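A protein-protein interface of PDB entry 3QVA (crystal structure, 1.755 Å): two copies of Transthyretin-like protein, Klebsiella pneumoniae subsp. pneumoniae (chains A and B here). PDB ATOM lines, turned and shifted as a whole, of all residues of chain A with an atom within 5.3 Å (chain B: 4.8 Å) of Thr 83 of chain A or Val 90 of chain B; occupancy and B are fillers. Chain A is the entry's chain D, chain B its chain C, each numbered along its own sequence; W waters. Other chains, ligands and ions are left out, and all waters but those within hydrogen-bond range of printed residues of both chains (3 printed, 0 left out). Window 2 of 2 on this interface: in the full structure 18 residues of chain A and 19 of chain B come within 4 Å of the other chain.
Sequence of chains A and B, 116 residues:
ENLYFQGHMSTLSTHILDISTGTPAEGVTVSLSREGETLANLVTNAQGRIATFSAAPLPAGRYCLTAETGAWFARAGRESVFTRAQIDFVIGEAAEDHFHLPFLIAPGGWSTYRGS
The backbone carbonyl oxygen (O) of Asp 88 of chain B is in hydrogen-bond range of the backbone NH (N) of Thr 83 of chain A, at 3.0 Å.
The guanidinium group (NH2) of Arg 84 of chain A is in salt-bridge range of the side-chain carboxylate (OD1) of Asp 88 of chain B (3.0 Å).
O of Val 81 of chain A is in hydrogen-bond range of N of Val 90 of chain B (2.9 Å).
Of the 8 printed residues of chain B, 5 touch a printed residue of chain A.
Of the 10 printed residues of chain A, 4 touch a printed residue of chain B.
Hydrophobic or aromatic side chains of chain A that line the printed part of chain B: Val 81 and Phe 82.
Among the printed residues, 9 pairs touch across the chains.
Among the printed residues, Asp or Glu carboxylates within 4 Å of a Lys or Arg side-chain nitrogen of the other chain: Arg 84 of chain A with Asp 88 of chain B (3.0 Å).
Of the printed residues of chain B, Phe 82 of chain A touches Asp 88 (3.4 Å).
Printed residues of chain A within 4 Å of Arg 62 of chain B: Thr 83 (3.5 Å).
The nearest residue of chain A that does not touch Val 90 of chain B is Ser 80 of chain A (4.1 Å).
O of Thr 83 of chain A is in hydrogen-bond range of N of Gly 70 of chain A, 3.2 Å away.
The side-chain hydroxyl (OG) of Ser 80 of chain A is in hydrogen-bond range of the backbone NH (N) of Phe 82 of chain A (3.1 Å).
No position is printed for both chains.
Of the 9 pairs that touch across the chains among the printed residues, none has its exchanged pair printed and touching as well.
Water W1 lies within hydrogen-bond range of the backbone carbonyl oxygen of Arg 84 of chain A (2.7 Å) and the backbone NH of Asp 88 of chain B (2.9 Å).
Water W3 lies within hydrogen-bond range of OG1 of Thr 83 of chain A (2.8 Å) and O of Phe 89 of chain B (2.9 Å).
Water W2 lies within hydrogen-bond range of O of Thr 83 of chain A and NH1 of Arg 62 of chain B.
Among the printed residues, merely in contact across the chains: Val 81 of chain A with Phe 89 of chain B, Val 81 of chain A with Phe 99 of chain B, Phe 82 of chain A with Asp 88 of chain B, Thr 83 of chain A with Arg 62 of chain B, Thr 83 of chain A with Phe 89 of chain B and Thr 83 of chain A with Val 90 of chain B.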
ATOM      1  N   GLU A  68      25.309  22.034  -0.695  1.00  0.00           N
ATOM      2  CA  GLU A  68      24.484  22.003   0.502  1.00  0.00           C
ATOM      3  C   GLU A  68      25.187  21.264   1.645  1.00  0.00           C
ATOM      4  O   GLU A  68      24.767  20.180   2.071  1.00  0.00           O
ATOM      5  CB  GLU A  68      23.113  21.400   0.199  1.00  0.00           C
ATOM      6  CG  GLU A  68      22.258  22.266  -0.709  1.00  0.00           C
ATOM      7  CD  GLU A  68      21.935  23.619  -0.093  1.00  0.00           C
ATOM      8  OE1 GLU A  68      21.576  23.674   1.105  1.00  0.00           O
ATOM      9  OE2 GLU A  68      22.032  24.634  -0.810  1.00  0.00           O
ATOM     10  N   THR A  69      26.240  21.881   2.164  1.00  0.00           N
ATOM     11  CA  THR A  69      27.105  21.217   3.141  1.00  0.00           C
ATOM     12  C   THR A  69      26.461  21.082   4.519  1.00  0.00           C
ATOM     13  O   THR A  69      26.589  20.040   5.165  1.00  0.00           O
ATOM     14  CB  THR A  69      28.469  21.923   3.263  1.00  0.00           C
ATOM     15  OG1 THR A  69      28.270  23.304   3.575  1.00  0.00           O
ATOM     16  CG2 THR A  69      29.245  21.808   1.944  1.00  0.00           C
ATOM     17  N   GLY A  70      25.775  22.133   4.964  1.00  0.00           N
ATOM     18  CA  GLY A  70      25.093  22.115   6.263  1.00  0.00           C
ATOM     19  C   GLY A  70      24.093  20.976   6.342  1.00  0.00           C
ATOM     20  O   GLY A  70      24.056  20.239   7.335  1.00  0.00           O
ATOM     21  N   ALA A  71      23.301  20.817   5.284  1.00  0.00           N
ATOM     22  CA  ALA A  71      22.313  19.737   5.213  1.00  0.00           C
ATOM     23  C   ALA A  71      22.987  18.366   5.193  1.00  0.00           C
ATOM     24  O   ALA A  71      22.497  17.420   5.808  1.00  0.00           O
ATOM     25  CB  ALA A  71      21.420  19.906   3.985  1.00  0.00           C
ATOM     26  N   SER A  80      27.229  22.064  12.412  1.00  0.00           N
ATOM     27  CA  SER A  80      28.174  22.991  11.784  1.00  0.00           C
ATOM     28  C   SER A  80      27.597  24.393  11.790  1.00  0.00           C
ATOM     29  O   SER A  80      26.409  24.562  11.533  1.00  0.00           O
ATOM     30  CB  SER A  80      28.467  22.574  10.344  1.00  0.00           C
ATOM     31  OG  SER A  80      29.326  23.523   9.728  1.00  0.00           O
ATOM     32  N   VAL A  81      28.430  25.393  12.074  1.00  0.00           N
ATOM     33  CA  VAL A  81      27.983  26.788  11.982  1.00  0.00           C
ATOM     34  C   VAL A  81      27.827  27.251  10.530  1.00  0.00           C
ATOM     35  O   VAL A  81      27.156  28.242  10.271  1.00  0.00           O
ATOM     36  CB  VAL A  81      28.881  27.795  12.771  1.00  0.00           C
ATOM     37  CG1 VAL A  81      28.849  27.493  14.282  1.00  0.00           C
ATOM     38  CG2 VAL A  81      30.310  27.853  12.207  1.00  0.00           C
ATOM     39  N   PHE A  82      28.437  26.534   9.592  1.00  0.00           N
ATOM     40  CA  PHE A  82      28.281  26.879   8.173  1.00  0.00           C
ATOM     41  C   PHE A  82      27.082  26.159   7.586  1.00  0.00           C
ATOM     42  O   PHE A  82      26.978  24.937   7.675  1.00  0.00           O
ATOM     43  CB  PHE A  82      29.560  26.586   7.381  1.00  0.00           C
ATOM     44  CG  PHE A  82      30.770  27.310   7.915  1.00  0.00           C
ATOM     45  CD1 PHE A  82      31.700  26.643   8.703  1.00  0.00           C
ATOM     46  CD2 PHE A  82      30.959  28.664   7.659  1.00  0.00           C
ATOM     47  CE1 PHE A  82      32.811  27.311   9.224  1.00  0.00           C
ATOM     48  CE2 PHE A  82      32.076  29.342   8.177  1.00  0.00           C
ATOM     49  CZ  PHE A  82      33.003  28.654   8.955  1.00  0.00           C
ATOM     50  N   THR A  83      26.174  26.924   6.986  1.00  0.00           N
ATOM     51  CA  THR A  83      24.901  26.377   6.525  1.00  0.00           C
ATOM     52  C   THR A  83      24.990  25.801   5.118  1.00  0.00           C
ATOM     53  O   THR A  83      24.237  24.896   4.763  1.00  0.00           O
ATOM     54  CB  THR A  83      23.764  27.420   6.601  1.00  0.00           C
ATOM     55  OG1 THR A  83      24.087  28.552   5.787  1.00  0.00           O
ATOM     56  CG2 THR A  83      23.553  27.881   8.033  1.00  0.00           C
ATOM     57  N   ARG A  84      25.923  26.325   4.329  1.00  0.00           N
ATOM     58  CA  ARG A  84      26.114  25.920   2.940  1.00  0.00           C
ATOM     59  C   ARG A  84      27.449  26.511   2.495  1.00  0.00           C
ATOM     60  O   ARG A  84      28.041  27.319   3.216  1.00  0.00           O
ATOM     61  CB  ARG A  84      24.986  26.470   2.061  1.00  0.00           C
ATOM     62  CG  ARG A  84      24.961  27.987   2.026  1.00  0.00           C
ATOM     63  CD  ARG A  84      23.563  28.560   1.918  1.00  0.00           C
ATOM     64  NE  ARG A  84      23.053  28.579   0.552  1.00  0.00           N
ATOM     65  CZ  ARG A  84      23.352  29.506  -0.357  1.00  0.00           C
ATOM     66  NH1 ARG A  84      22.821  29.432  -1.572  1.00  0.00           N
ATOM     67  NH2 ARG A  84      24.190  30.499  -0.066  1.00  0.00           N
ATOM     68  N   ALA A  85      27.905  26.119   1.313  1.00  0.00           N
ATOM     69  CA  ALA A  85      29.143  26.640   0.747  1.00  0.00           C
ATOM     70  C   ALA A  85      28.883  27.118  -0.681  1.00  0.00           C
ATOM     71  O   ALA A  85      28.645  26.318  -1.584  1.00  0.00           O
ATOM     72  CB  ALA A  85      30.223  25.570   0.776  1.00  0.00           C
ATOM     73  N   GLY B  61      19.814  33.480  14.145  1.00  0.00           N
ATOM     74  CA  GLY B  61      19.341  33.574  12.771  1.00  0.00           C
ATOM     75  C   GLY B  61      20.406  33.164  11.778  1.00  0.00           C
ATOM     76  O   GLY B  61      21.505  32.761  12.166  1.00  0.00           O
ATOM     77  N   ARG B  62      20.070  33.261  10.495  1.00  0.00           N
ATOM     78  CA  ARG B  62      20.994  32.897   9.427  1.00  0.00           C
ATOM     79  C   ARG B  62      21.587  34.148   8.802  1.00  0.00           C
ATOM     80  O   ARG B  62      20.864  35.074   8.422  1.00  0.00           O
ATOM     81  CB  ARG B  62      20.303  32.018   8.381  1.00  0.00           C
ATOM     82  CG  ARG B  62      20.060  30.599   8.886  1.00  0.00           C
ATOM     83  CD  ARG B  62      19.166  29.809   7.952  1.00  0.00           C
ATOM     84  NE  ARG B  62      18.781  28.542   8.571  1.00  0.00           N
ATOM     85  CZ  ARG B  62      19.293  27.357   8.250  1.00  0.00           C
ATOM     86  NH1 ARG B  62      20.206  27.249   7.292  1.00  0.00           N
ATOM     87  NH2 ARG B  62      18.875  26.270   8.882  1.00  0.00           N
ATOM     88  N   ASP B  88      28.165  31.720   4.602  1.00  0.00           N
ATOM     89  CA  ASP B  88      26.797  31.593   5.099  1.00  0.00           C
ATOM     90  C   ASP B  88      26.847  30.805   6.390  1.00  0.00           C
ATOM     91  O   ASP B  88      27.333  29.677   6.413  1.00  0.00           O
ATOM     92  CB  ASP B  88      25.924  30.879   4.067  1.00  0.00           C
ATOM     93  CG  ASP B  88      25.703  31.713   2.826  1.00  0.00           C
ATOM     94  OD1 ASP B  88      26.342  31.413   1.791  1.00  0.00           O
ATOM     95  OD2 ASP B  88      24.909  32.686   2.900  1.00  0.00           O
ATOM     96  N   PHE B  89      26.372  31.413   7.470  1.00  0.00           N
ATOM     97  CA  PHE B  89      26.479  30.787   8.779  1.00  0.00           C
ATOM     98  C   PHE B  89      25.231  31.010   9.617  1.00  0.00           C
ATOM     99  O   PHE B  89      24.352  31.800   9.253  1.00  0.00           O
ATOM    100  CB  PHE B  89      27.749  31.251   9.513  1.00  0.00           C
ATOM    101  CG  PHE B  89      27.737  32.702   9.917  1.00  0.00           C
ATOM    102  CD1 PHE B  89      27.476  33.063  11.233  1.00  0.00           C
ATOM    103  CD2 PHE B  89      28.007  33.706   8.985  1.00  0.00           C
ATOM    104  CE1 PHE B  89      27.474  34.410  11.622  1.00  0.00           C
ATOM    105  CE2 PHE B  89      28.006  35.053   9.361  1.00  0.00           C
ATOM    106  CZ  PHE B  89      27.746  35.403  10.681  1.00  0.00           C
ATOM    107  N   VAL B  90      25.155  30.290  10.729  1.00  0.00           N
ATOM    108  CA  VAL B  90      24.000  30.376  11.606  1.00  0.00           C
ATOM    109  C   VAL B  90      24.427  30.686  13.034  1.00  0.00           C
ATOM    110  O   VAL B  90      25.367  30.088  13.561  1.00  0.00           O
ATOM    111  CB  VAL B  90      23.134  29.079  11.543  1.00  0.00           C
ATOM    112  CG1 VAL B  90      23.954  27.834  11.931  1.00  0.00           C
ATOM    113  CG2 VAL B  90      21.877  29.221  12.400  1.00  0.00           C
ATOM    114  N   ILE B  91      23.734  31.642  13.642  1.00  0.00           N
ATOM    115  CA  ILE B  91      23.840  31.875  15.079  1.00  0.00           C
ATOM    116  C   ILE B  91      22.675  31.140  15.750  1.00  0.00           C
ATOM    117  O   ILE B  91      21.502  31.419  15.477  1.00  0.00           O
ATOM    118  CB  ILE B  91      23.871  33.386  15.412  1.00  0.00           C
ATOM    119  CG1 ILE B  91      25.084  34.039  14.730  1.00  0.00           C
ATOM    120  CG2 ILE B  91      23.911  33.608  16.925  1.00  0.00           C
ATOM    121  CD1 ILE B  91      25.168  35.551  14.843  1.00  0.00           C
ATOM    122  N   GLY B  92      23.016  30.168  16.591  1.00  0.00           N
ATOM    123  CA  GLY B  92      22.030  29.303  17.236  1.00  0.00           C
ATOM    124  C   GLY B  92      21.555  29.861  18.561  1.00  0.00           C
ATOM    125  O   GLY B  92      21.555  31.079  18.761  1.00  0.00           O
ATOM    126  N   PHE B  99      31.733  35.004  17.369  1.00  0.00           N
ATOM    127  CA  PHE B  99      32.055  34.327  16.121  1.00  0.00           C
ATOM    128  C   PHE B  99      33.165  35.096  15.424  1.00  0.00           C
ATOM    129  O   PHE B  99      32.984  36.268  15.075  1.00  0.00           O
ATOM    130  CB  PHE B  99      30.836  34.282  15.192  1.00  0.00           C
ATOM    131  CG  PHE B  99      29.782  33.304  15.608  1.00  0.00           C
ATOM    132  CD1 PHE B  99      28.949  33.574  16.687  1.00  0.00           C
ATOM    133  CD2 PHE B  99      29.601  32.119  14.903  1.00  0.00           C
ATOM    134  CE1 PHE B  99      27.963  32.662  17.070  1.00  0.00           C
ATOM    135  CE2 PHE B  99      28.615  31.200  15.281  1.00  0.00           C
ATOM    136  CZ  PHE B  99      27.798  31.476  16.366  1.00  0.00           C
HETATM  137  O   HOH W   1      29.616  29.319   4.032  1.00  0.00           O
HETATM  138  O   HOH W   2      21.554  24.283   6.163  1.00  0.00           O
HETATM  139  O   HOH W   3      23.230  30.998   6.744  1.00  0.00           O
